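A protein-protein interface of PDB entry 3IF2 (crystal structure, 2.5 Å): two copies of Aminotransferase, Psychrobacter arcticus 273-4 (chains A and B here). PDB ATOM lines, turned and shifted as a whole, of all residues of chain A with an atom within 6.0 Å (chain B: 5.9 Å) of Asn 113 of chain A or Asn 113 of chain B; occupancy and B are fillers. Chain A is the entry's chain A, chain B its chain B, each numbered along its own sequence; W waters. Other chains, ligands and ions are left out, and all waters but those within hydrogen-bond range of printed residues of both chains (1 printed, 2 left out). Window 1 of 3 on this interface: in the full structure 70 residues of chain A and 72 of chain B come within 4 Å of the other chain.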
ATOM      1  N   LEU A 111      -0.297  12.765 -32.525  1.00  0.00           N
ATOM      2  CA  LEU A 111      -1.633  13.229 -32.187  1.00  0.00           C
ATOM      3  C   LEU A 111      -1.540  14.096 -30.920  1.00  0.00           C
ATOM      4  O   LEU A 111      -0.673  13.849 -30.045  1.00  0.00           O
ATOM      5  CB  LEU A 111      -2.584  12.043 -31.949  1.00  0.00           C
ATOM      6  CG  LEU A 111      -2.774  11.018 -33.071  1.00  0.00           C
ATOM      7  CD1 LEU A 111      -3.757   9.906 -32.650  1.00  0.00           C
ATOM      8  CD2 LEU A 111      -3.259  11.688 -34.302  1.00  0.00           C
ATOM      9  N   THR A 112      -2.424  15.104 -30.848  1.00  0.00           N
ATOM     10  CA  THR A 112      -2.550  16.024 -29.710  1.00  0.00           C
ATOM     11  C   THR A 112      -4.036  16.138 -29.322  1.00  0.00           C
ATOM     12  O   THR A 112      -4.902  15.661 -30.063  1.00  0.00           O
ATOM     13  CB  THR A 112      -1.957  17.427 -30.064  1.00  0.00           C
ATOM     14  OG1 THR A 112      -2.681  18.022 -31.158  1.00  0.00           O
ATOM     15  CG2 THR A 112      -0.489  17.313 -30.452  1.00  0.00           C
ATOM     16  N   ASN A 113      -4.325  16.742 -28.167  1.00  0.00           N
ATOM     17  CA  ASN A 113      -5.705  16.948 -27.691  1.00  0.00           C
ATOM     18  C   ASN A 113      -6.327  18.197 -28.350  1.00  0.00           C
ATOM     19  O   ASN A 113      -6.615  19.183 -27.684  1.00  0.00           O
ATOM     20  CB  ASN A 113      -5.763  17.033 -26.151  1.00  0.00           C
ATOM     21  CG  ASN A 113      -5.434  15.703 -25.463  1.00  0.00           C
ATOM     22  OD1 ASN A 113      -5.631  14.619 -26.025  1.00  0.00           O
ATOM     23  ND2 ASN A 113      -4.943  15.791 -24.221  1.00  0.00           N
ATOM     24  N   GLY A 114      -6.588  18.088 -29.659  1.00  0.00           N
ATOM     25  CA  GLY A 114      -7.033  19.185 -30.534  1.00  0.00           C
ATOM     26  C   GLY A 114      -5.804  19.925 -31.078  1.00  0.00           C
ATOM     27  O   GLY A 114      -4.702  19.803 -30.521  1.00  0.00           O
ATOM     28  N   SER A 115      -5.957  20.657 -32.183  1.00  0.00           N
ATOM     29  CA  SER A 115      -4.844  21.453 -32.749  1.00  0.00           C
ATOM     30  C   SER A 115      -4.366  22.565 -31.810  1.00  0.00           C
ATOM     31  O   SER A 115      -3.233  22.975 -31.896  1.00  0.00           O
ATOM     32  CB  SER A 115      -5.194  22.031 -34.123  1.00  0.00           C
ATOM     33  OG  SER A 115      -5.124  21.010 -35.091  1.00  0.00           O
ATOM     34  N   GLN A 116      -5.235  23.035 -30.903  1.00  0.00           N
ATOM     35  CA  GLN A 116      -4.871  24.054 -29.897  1.00  0.00           C
ATOM     36  C   GLN A 116      -3.712  23.550 -29.008  1.00  0.00           C
ATOM     37  O   GLN A 116      -2.773  24.294 -28.692  1.00  0.00           O
ATOM     38  CB  GLN A 116      -6.077  24.402 -29.015  1.00  0.00           C
ATOM     39  CG  GLN A 116      -5.867  25.598 -28.034  1.00  0.00           C
ATOM     40  CD  GLN A 116      -5.676  26.925 -28.728  1.00  0.00           C
ATOM     41  OE1 GLN A 116      -6.092  27.104 -29.881  1.00  0.00           O
ATOM     42  NE2 GLN A 116      -5.066  27.873 -28.024  1.00  0.00           N
ATOM     43  N   ASN A 117      -3.807  22.277 -28.617  1.00  0.00           N
ATOM     44  CA  ASN A 117      -2.770  21.581 -27.862  1.00  0.00           C
ATOM     45  C   ASN A 117      -1.493  21.554 -28.712  1.00  0.00           C
ATOM     46  O   ASN A 117      -0.391  21.786 -28.201  1.00  0.00           O
ATOM     47  CB  ASN A 117      -3.280  20.163 -27.543  1.00  0.00           C
ATOM     48  CG  ASN A 117      -2.639  19.528 -26.341  1.00  0.00           C
ATOM     49  OD1 ASN A 117      -2.408  18.313 -26.320  1.00  0.00           O
ATOM     50  ND2 ASN A 117      -2.429  20.312 -25.305  1.00  0.00           N
ATOM     51  N   ALA A 118      -1.645  21.316 -30.017  1.00  0.00           N
ATOM     52  CA  ALA A 118      -0.509  21.361 -30.944  1.00  0.00           C
ATOM     53  C   ALA A 118       0.164  22.749 -30.952  1.00  0.00           C
ATOM     54  O   ALA A 118       1.386  22.823 -30.923  1.00  0.00           O
ATOM     55  CB  ALA A 118      -0.914  20.952 -32.354  1.00  0.00           C
ATOM     56  N   ARG A 283     -11.639  16.322 -29.445  1.00  0.00           N
ATOM     57  CA  ARG A 283     -10.323  16.930 -29.246  1.00  0.00           C
ATOM     58  C   ARG A 283      -9.184  16.138 -29.866  1.00  0.00           C
ATOM     59  O   ARG A 283      -8.337  15.623 -29.146  1.00  0.00           O
ATOM     60  CB  ARG A 283     -10.040  17.183 -27.736  1.00  0.00           C
ATOM     61  CG  ARG A 283     -11.157  17.812 -26.883  1.00  0.00           C
ATOM     62  CD  ARG A 283     -11.346  19.324 -27.023  1.00  0.00           C
ATOM     63  NE  ARG A 283     -11.443  19.683 -28.396  1.00  0.00           N
ATOM     64  CZ  ARG A 283     -10.612  20.436 -29.116  1.00  0.00           C
ATOM     65  NH1 ARG A 283      -9.605  21.177 -28.617  1.00  0.00           N
ATOM     66  NH2 ARG A 283     -10.897  20.494 -30.401  1.00  0.00           N
ATOM     67  N   THR A 284      -9.157  16.056 -31.199  1.00  0.00           N
ATOM     68  CA  THR A 284      -8.074  15.349 -31.928  1.00  0.00           C
ATOM     69  C   THR A 284      -7.366  16.271 -32.912  1.00  0.00           C
ATOM     70  O   THR A 284      -7.980  16.718 -33.893  1.00  0.00           O
ATOM     71  CB  THR A 284      -8.596  14.139 -32.716  1.00  0.00           C
ATOM     72  OG1 THR A 284      -9.429  13.359 -31.860  1.00  0.00           O
ATOM     73  CG2 THR A 284      -7.426  13.296 -33.253  1.00  0.00           C
ATOM     74  N   GLY A 285      -6.095  16.560 -32.621  1.00  0.00           N
ATOM     75  CA  GLY A 285      -5.206  17.319 -33.502  1.00  0.00           C
ATOM     76  C   GLY A 285      -4.221  16.333 -34.123  1.00  0.00           C
ATOM     77  O   GLY A 285      -3.868  15.346 -33.484  1.00  0.00           O
ATOM     78  N   ASN A 301       3.592  15.323 -24.677  1.00  0.00           N
ATOM     79  CA  ASN A 301       2.349  14.574 -24.375  1.00  0.00           C
ATOM     80  C   ASN A 301       2.523  13.720 -23.148  1.00  0.00           C
ATOM     81  O   ASN A 301       1.702  13.789 -22.261  1.00  0.00           O
ATOM     82  CB  ASN A 301       1.876  13.679 -25.558  1.00  0.00           C
ATOM     83  CG  ASN A 301       0.992  14.421 -26.563  1.00  0.00           C
ATOM     84  OD1 ASN A 301       0.337  15.407 -26.228  1.00  0.00           O
ATOM     85  ND2 ASN A 301       0.906  13.891 -27.772  1.00  0.00           N
ATOM     86  N   VAL A 304       2.668  16.315 -20.027  1.00  0.00           N
ATOM     87  CA  VAL A 304       1.458  17.138 -19.873  1.00  0.00           C
ATOM     88  C   VAL A 304       0.170  16.341 -19.848  1.00  0.00           C
ATOM     89  O   VAL A 304      -0.732  16.687 -19.076  1.00  0.00           O
ATOM     90  CB  VAL A 304       1.359  18.199 -20.989  1.00  0.00           C
ATOM     91  CG1 VAL A 304       0.062  19.045 -20.861  1.00  0.00           C
ATOM     92  CG2 VAL A 304       2.605  19.116 -20.950  1.00  0.00           C
ATOM     93  N   ASN A 305       0.106  15.268 -20.644  1.00  0.00           N
ATOM     94  CA  ASN A 305      -1.120  14.482 -20.850  1.00  0.00           C
ATOM     95  C   ASN A 305      -1.095  12.982 -20.574  1.00  0.00           C
ATOM     96  O   ASN A 305      -2.160  12.358 -20.586  1.00  0.00           O
ATOM     97  CB  ASN A 305      -1.512  14.632 -22.339  1.00  0.00           C
ATOM     98  CG  ASN A 305      -1.855  16.046 -22.719  1.00  0.00           C
ATOM     99  OD1 ASN A 305      -2.455  16.773 -21.936  1.00  0.00           O
ATOM    100  ND2 ASN A 305      -1.528  16.427 -23.948  1.00  0.00           N
ATOM    101  N   ALA A 307      -0.982  10.463 -22.282  1.00  0.00           N
ATOM    102  CA  ALA A 307      -1.208  10.113 -23.694  1.00  0.00           C
ATOM    103  C   ALA A 307      -2.366  10.981 -24.212  1.00  0.00           C
ATOM    104  O   ALA A 307      -3.156  11.486 -23.425  1.00  0.00           O
ATOM    105  CB  ALA A 307      -1.518   8.632 -23.860  1.00  0.00           C
ATOM    106  N   PRO A 308      -2.430  11.223 -25.519  1.00  0.00           N
ATOM    107  CA  PRO A 308      -3.549  12.014 -25.970  1.00  0.00           C
ATOM    108  C   PRO A 308      -4.817  11.161 -26.034  1.00  0.00           C
ATOM    109  O   PRO A 308      -4.793   9.929 -25.909  1.00  0.00           O
ATOM    110  CB  PRO A 308      -3.112  12.509 -27.357  1.00  0.00           C
ATOM    111  CG  PRO A 308      -1.983  11.639 -27.776  1.00  0.00           C
ATOM    112  CD  PRO A 308      -1.615  10.739 -26.642  1.00  0.00           C
ATOM    113  N   THR A 309      -5.915  11.856 -26.253  1.00  0.00           N
ATOM    114  CA  THR A 309      -7.241  11.250 -26.363  1.00  0.00           C
ATOM    115  C   THR A 309      -7.302  10.329 -27.568  1.00  0.00           C
ATOM    116  O   THR A 309      -6.527  10.504 -28.512  1.00  0.00           O
ATOM    117  CB  THR A 309      -8.310  12.348 -26.418  1.00  0.00           C
ATOM    118  OG1 THR A 309      -9.546  11.780 -26.038  1.00  0.00           O
ATOM    119  CG2 THR A 309      -8.403  12.982 -27.768  1.00  0.00           C
ATOM    120  N   LEU B 111     -13.070  19.859 -15.482  1.00  0.00           N
ATOM    121  CA  LEU B 111     -12.595  18.664 -16.165  1.00  0.00           C
ATOM    122  C   LEU B 111     -11.310  19.006 -16.884  1.00  0.00           C
ATOM    123  O   LEU B 111     -11.153  20.136 -17.354  1.00  0.00           O
ATOM    124  CB  LEU B 111     -13.626  18.144 -17.191  1.00  0.00           C
ATOM    125  CG  LEU B 111     -15.034  17.794 -16.703  1.00  0.00           C
ATOM    126  CD1 LEU B 111     -15.838  17.243 -17.887  1.00  0.00           C
ATOM    127  CD2 LEU B 111     -15.032  16.834 -15.504  1.00  0.00           C
ATOM    128  N   THR B 112     -10.407  18.019 -16.968  1.00  0.00           N
ATOM    129  CA  THR B 112      -9.112  18.120 -17.664  1.00  0.00           C
ATOM    130  C   THR B 112      -8.890  16.867 -18.530  1.00  0.00           C
ATOM    131  O   THR B 112      -9.618  15.896 -18.393  1.00  0.00           O
ATOM    132  CB  THR B 112      -7.960  18.242 -16.634  1.00  0.00           C
ATOM    133  OG1 THR B 112      -7.995  17.119 -15.723  1.00  0.00           O
ATOM    134  CG2 THR B 112      -8.091  19.533 -15.845  1.00  0.00           C
ATOM    135  N   ASN B 113      -7.884  16.885 -19.399  1.00  0.00           N
ATOM    136  CA  ASN B 113      -7.556  15.727 -20.254  1.00  0.00           C
ATOM    137  C   ASN B 113      -6.755  14.666 -19.494  1.00  0.00           C
ATOM    138  O   ASN B 113      -5.605  14.381 -19.821  1.00  0.00           O
ATOM    139  CB  ASN B 113      -6.854  16.181 -21.538  1.00  0.00           C
ATOM    140  CG  ASN B 113      -7.754  17.028 -22.398  1.00  0.00           C
ATOM    141  OD1 ASN B 113      -8.979  16.893 -22.321  1.00  0.00           O
ATOM    142  ND2 ASN B 113      -7.169  17.917 -23.213  1.00  0.00           N
ATOM    143  N   GLY B 114      -7.433  14.041 -18.530  1.00  0.00           N
ATOM    144  CA  GLY B 114      -6.836  13.097 -17.572  1.00  0.00           C
ATOM    145  C   GLY B 114      -6.311  13.872 -16.361  1.00  0.00           C
ATOM    146  O   GLY B 114      -6.072  15.091 -16.463  1.00  0.00           O
ATOM    147  N   SER B 115      -6.161  13.190 -15.222  1.00  0.00           N
ATOM    148  CA  SER B 115      -5.592  13.795 -14.004  1.00  0.00           C
ATOM    149  C   SER B 115      -4.198  14.370 -14.222  1.00  0.00           C
ATOM    150  O   SER B 115      -3.851  15.371 -13.592  1.00  0.00           O
ATOM    151  CB  SER B 115      -5.532  12.797 -12.854  1.00  0.00           C
ATOM    152  OG  SER B 115      -6.774  12.703 -12.208  1.00  0.00           O
ATOM    153  N   GLN B 116      -3.430  13.746 -15.126  1.00  0.00           N
ATOM    154  CA  GLN B 116      -2.076  14.190 -15.485  1.00  0.00           C
ATOM    155  C   GLN B 116      -2.062  15.642 -15.949  1.00  0.00           C
ATOM    156  O   GLN B 116      -1.183  16.414 -15.554  1.00  0.00           O
ATOM    157  CB  GLN B 116      -1.477  13.298 -16.574  1.00  0.00           C
ATOM    158  CG  GLN B 116       0.040  13.544 -16.888  1.00  0.00           C
ATOM    159  CD  GLN B 116       0.973  13.221 -15.718  1.00  0.00           C
ATOM    160  OE1 GLN B 116       0.621  12.465 -14.803  1.00  0.00           O
ATOM    161  NE2 GLN B 116       2.167  13.773 -15.757  1.00  0.00           N
ATOM    162  N   ASN B 117      -3.064  16.000 -16.751  1.00  0.00           N
ATOM    163  CA  ASN B 117      -3.295  17.366 -17.221  1.00  0.00           C
ATOM    164  C   ASN B 117      -3.639  18.282 -16.036  1.00  0.00           C
ATOM    165  O   ASN B 117      -3.169  19.420 -15.982  1.00  0.00           O
ATOM    166  CB  ASN B 117      -4.393  17.343 -18.319  1.00  0.00           C
ATOM    167  CG  ASN B 117      -4.546  18.661 -19.090  1.00  0.00           C
ATOM    168  OD1 ASN B 117      -5.640  18.973 -19.572  1.00  0.00           O
ATOM    169  ND2 ASN B 117      -3.469  19.407 -19.236  1.00  0.00           N
ATOM    170  N   ALA B 118      -4.419  17.772 -15.079  1.00  0.00           N
ATOM    171  CA  ALA B 118      -4.726  18.493 -13.837  1.00  0.00           C
ATOM    172  C   ALA B 118      -3.482  18.774 -12.979  1.00  0.00           C
ATOM    173  O   ALA B 118      -3.420  19.813 -12.352  1.00  0.00           O
ATOM    174  CB  ALA B 118      -5.783  17.771 -12.992  1.00  0.00           C
ATOM    175  N   ARG B 283      -9.316   9.881 -21.281  1.00  0.00           N
ATOM    176  CA  ARG B 283      -8.549  11.044 -20.765  1.00  0.00           C
ATOM    177  C   ARG B 283      -9.461  12.055 -20.094  1.00  0.00           C
ATOM    178  O   ARG B 283      -9.638  13.167 -20.593  1.00  0.00           O
ATOM    179  CB  ARG B 283      -7.700  11.747 -21.860  1.00  0.00           C
ATOM    180  CG  ARG B 283      -6.940  10.849 -22.866  1.00  0.00           C
ATOM    181  CD  ARG B 283      -5.641  10.287 -22.433  1.00  0.00           C
ATOM    182  NE  ARG B 283      -5.798   9.685 -21.154  1.00  0.00           N
ATOM    183  CZ  ARG B 283      -5.227  10.037 -20.001  1.00  0.00           C
ATOM    184  NH1 ARG B 283      -4.261  10.947 -19.879  1.00  0.00           N
ATOM    185  NH2 ARG B 283      -5.618   9.372 -18.939  1.00  0.00           N
ATOM    186  N   THR B 284     -10.024  11.659 -18.955  1.00  0.00           N
ATOM    187  CA  THR B 284     -10.915  12.520 -18.181  1.00  0.00           C
ATOM    188  C   THR B 284     -10.486  12.602 -16.720  1.00  0.00           C
ATOM    189  O   THR B 284     -10.614  11.624 -16.000  1.00  0.00           O
ATOM    190  CB  THR B 284     -12.370  12.029 -18.221  1.00  0.00           C
ATOM    191  OG1 THR B 284     -12.781  11.816 -19.578  1.00  0.00           O
ATOM    192  CG2 THR B 284     -13.278  13.055 -17.535  1.00  0.00           C
ATOM    193  N   GLY B 285      -9.978  13.774 -16.314  1.00  0.00           N
ATOM    194  CA  GLY B 285      -9.675  14.097 -14.930  1.00  0.00           C
ATOM    195  C   GLY B 285     -10.783  15.028 -14.416  1.00  0.00           C
ATOM    196  O   GLY B 285     -11.397  15.747 -15.210  1.00  0.00           O
ATOM    197  N   ASN B 301      -7.451  25.623 -19.456  1.00  0.00           N
ATOM    198  CA  ASN B 301      -8.078  24.779 -20.508  1.00  0.00           C
ATOM    199  C   ASN B 301      -8.363  25.584 -21.766  1.00  0.00           C
ATOM    200  O   ASN B 301      -8.017  25.143 -22.846  1.00  0.00           O
ATOM    201  CB  ASN B 301      -9.397  24.126 -20.051  1.00  0.00           C
ATOM    202  CG  ASN B 301      -9.207  22.796 -19.336  1.00  0.00           C
ATOM    203  OD1 ASN B 301      -8.231  22.079 -19.564  1.00  0.00           O
ATOM    204  ND2 ASN B 301     -10.189  22.424 -18.524  1.00  0.00           N
ATOM    205  N   VAL B 304      -4.613  26.252 -23.368  1.00  0.00           N
ATOM    206  CA  VAL B 304      -3.842  25.051 -23.713  1.00  0.00           C
ATOM    207  C   VAL B 304      -4.633  24.036 -24.528  1.00  0.00           C
ATOM    208  O   VAL B 304      -4.056  23.436 -25.433  1.00  0.00           O
ATOM    209  CB  VAL B 304      -3.268  24.362 -22.439  1.00  0.00           C
ATOM    210  CG1 VAL B 304      -2.563  23.024 -22.781  1.00  0.00           C
ATOM    211  CG2 VAL B 304      -2.323  25.310 -21.720  1.00  0.00           C
ATOM    212  N   ASN B 305      -5.929  23.866 -24.228  1.00  0.00           N
ATOM    213  CA  ASN B 305      -6.805  22.848 -24.864  1.00  0.00           C
ATOM    214  C   ASN B 305      -8.049  23.302 -25.662  1.00  0.00           C
ATOM    215  O   ASN B 305      -8.675  22.478 -26.316  1.00  0.00           O
ATOM    216  CB  ASN B 305      -7.359  21.965 -23.739  1.00  0.00           C
ATOM    217  CG  ASN B 305      -6.303  21.171 -23.031  1.00  0.00           C
ATOM    218  OD1 ASN B 305      -5.312  20.740 -23.620  1.00  0.00           O
ATOM    219  ND2 ASN B 305      -6.534  20.940 -21.746  1.00  0.00           N
ATOM    220  N   ALA B 307     -11.066  23.361 -25.163  1.00  0.00           N
ATOM    221  CA  ALA B 307     -12.020  22.720 -24.264  1.00  0.00           C
ATOM    222  C   ALA B 307     -11.471  21.313 -23.910  1.00  0.00           C
ATOM    223  O   ALA B 307     -10.678  20.744 -24.652  1.00  0.00           O
ATOM    224  CB  ALA B 307     -13.395  22.639 -24.910  1.00  0.00           C
ATOM    225  N   PRO B 308     -11.790  20.792 -22.730  1.00  0.00           N
ATOM    226  CA  PRO B 308     -11.306  19.449 -22.463  1.00  0.00           C
ATOM    227  C   PRO B 308     -12.176  18.426 -23.189  1.00  0.00           C
ATOM    228  O   PRO B 308     -13.278  18.729 -23.683  1.00  0.00           O
ATOM    229  CB  PRO B 308     -11.424  19.318 -20.944  1.00  0.00           C
ATOM    230  CG  PRO B 308     -12.497  20.243 -20.562  1.00  0.00           C
ATOM    231  CD  PRO B 308     -12.425  21.390 -21.550  1.00  0.00           C
ATOM    232  N   THR B 309     -11.668  17.210 -23.223  1.00  0.00           N
ATOM    233  CA  THR B 309     -12.334  16.107 -23.893  1.00  0.00           C
ATOM    234  C   THR B 309     -13.657  15.789 -23.185  1.00  0.00           C
ATOM    235  O   THR B 309     -13.795  16.014 -21.991  1.00  0.00           O
ATOM    236  CB  THR B 309     -11.402  14.886 -23.965  1.00  0.00           C
ATOM    237  OG1 THR B 309     -11.801  14.086 -25.069  1.00  0.00           O
ATOM    238  CG2 THR B 309     -11.401  14.085 -22.695  1.00  0.00           C
HETATM  239  O   HOH W   1      -4.359  18.242 -23.035  1.00  0.00           O
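The side-chain amide nitrogen (ND2) of Asn 113 of chain B lies close to the side-chain amide oxygen (OD1) of Asn 305 of chain B (3.4 Å). The side-chain amide oxygen (OD1) of Asn 117 of chain B is in hydrogen-bond range of the side-chain amide nitrogen (ND2) of Asn 305 of chain B (3.1 Å). The backbone NH (N) of Thr 309 of chain A lies within hydrogen-bond range of the side-chain amide oxygen (OD1) of Asn 113 of chain A. The side-chain amide nitrogen of Asn 305 of chain A sits close to the side-chain amide nitrogen of Asn 113 of chain A (3.5 Å). The backbone carbonyl oxygen of Arg 283 of chain B sits at hydrogen-bond distance from the backbone NH of Gly 114 of chain B (3.1 Å). ND2 of Asn 305 of chain B sits at hydrogen-bond distance from OD1 of Asn 301 of chain B (3.0 Å).
NH1 of Arg 283 of chain A lies within hydrogen-bond range of O of Asn 305 of chain B (2.8 Å). The backbone carbonyl oxygen (O) of Asn 305 of chain A lies within hydrogen-bond range of the guanidinium group (NH1) of Arg 283 of chain B (2.6 Å). OD1 of Asn 305 of chain B lies within hydrogen-bond range of ND2 of Asn 117 of chain A, at 3.4 Å. The side-chain amide nitrogen (ND2) of Asn 113 of chain B lies close to the side-chain amide nitrogen (ND2) of Asn 113 of chain A (3.2 Å). The backbone NH (N) of Asn 117 of chain A sits close to the backbone carbonyl oxygen (O) of Val 304 of chain B. The side-chain hydroxyl (OG1) of Thr 309 of chain B lies within hydrogen-bond range of the side-chain hydroxyl (OG1) of Thr 309 of chain A, at 3.4 Å. O of Val 304 of chain A sits close to N of Asn 117 of chain B, at 3.4 Å.
Among the printed residues, pairs that only touch across the chains: Gln 116 of chain A with Val 304 of chain B (3.6 Å), Gln 116 of chain A with Asn 305 of chain B (3.96 Å), Arg 283 of chain A with Ala 307 of chain B (2.8 Å), Arg 283 of chain A with Pro 308 of chain B (3.9 Å), Arg 283 of chain A with Thr 309 of chain B (3.6 Å), Val 304 of chain A with Gln 116 of chain B (3.6 Å), Asn 305 of chain A with Gln 116 of chain B (3.9 Å), Asn 305 of chain A with Asn 117 of chain B (3.9 Å), Ala 307 of chain A with Arg 283 of chain B (2.9 Å), Pro 308 of chain A with Arg 283 of chain B (3.6 Å) and Thr 309 of chain A with Arg 283 of chain B (3.5 Å).
Of the 17 printed residues of chain A, 9 touch a printed residue of chain B. Among the printed residues, no Asp or Glu carboxylate lies within 4 Å of a Lys or Arg side-chain nitrogen of the other chain.
Water W1 lies within hydrogen-bond range of the side-chain amide oxygen (OD1) of Asn 305 of chain A, the side-chain amide oxygen (OD1) of Asn 305 of chain B, the side-chain amide nitrogen (ND2) of Asn 113 of chain A and the side-chain amide nitrogen (ND2) of Asn 113 of chain B.
Asn 117 of chain A touches Asn 305 of chain B, and with the chains exchanged Asn 305 of chain A touches Asn 117 of chain B. Arg 283 of chain A touches Pro 308 of chain B, and with the chains exchanged Pro 308 of chain A touches Arg 283 of chain B. Arg 283 of chain A touches Thr 309 of chain B, and with the chains exchanged Thr 309 of chain A touches Arg 283 of chain B. Thr 309 of chain B touches its own counterpart, Thr 309 of chain A. 17 positions are printed for both chains.
Of the printed residues of chain B, Asn 117 of chain A touches Val 304 and Asn 305. Of the printed residues of chain B, Val 304 of chain A touches Gln 116 (3.6 Å) and Asn 117 (3.2 Å). Of chain A, only Asn 113 (3.2 Å) comes within 4 Å of Asn 113 of chain B. Of the printed residues of chain A, Val 304 of chain B touches Gln 116 and Asn 117. The nearest printed residue of chain B that does not touch Thr 309 of chain A is Asn 113 of chain B (6.2 Å).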
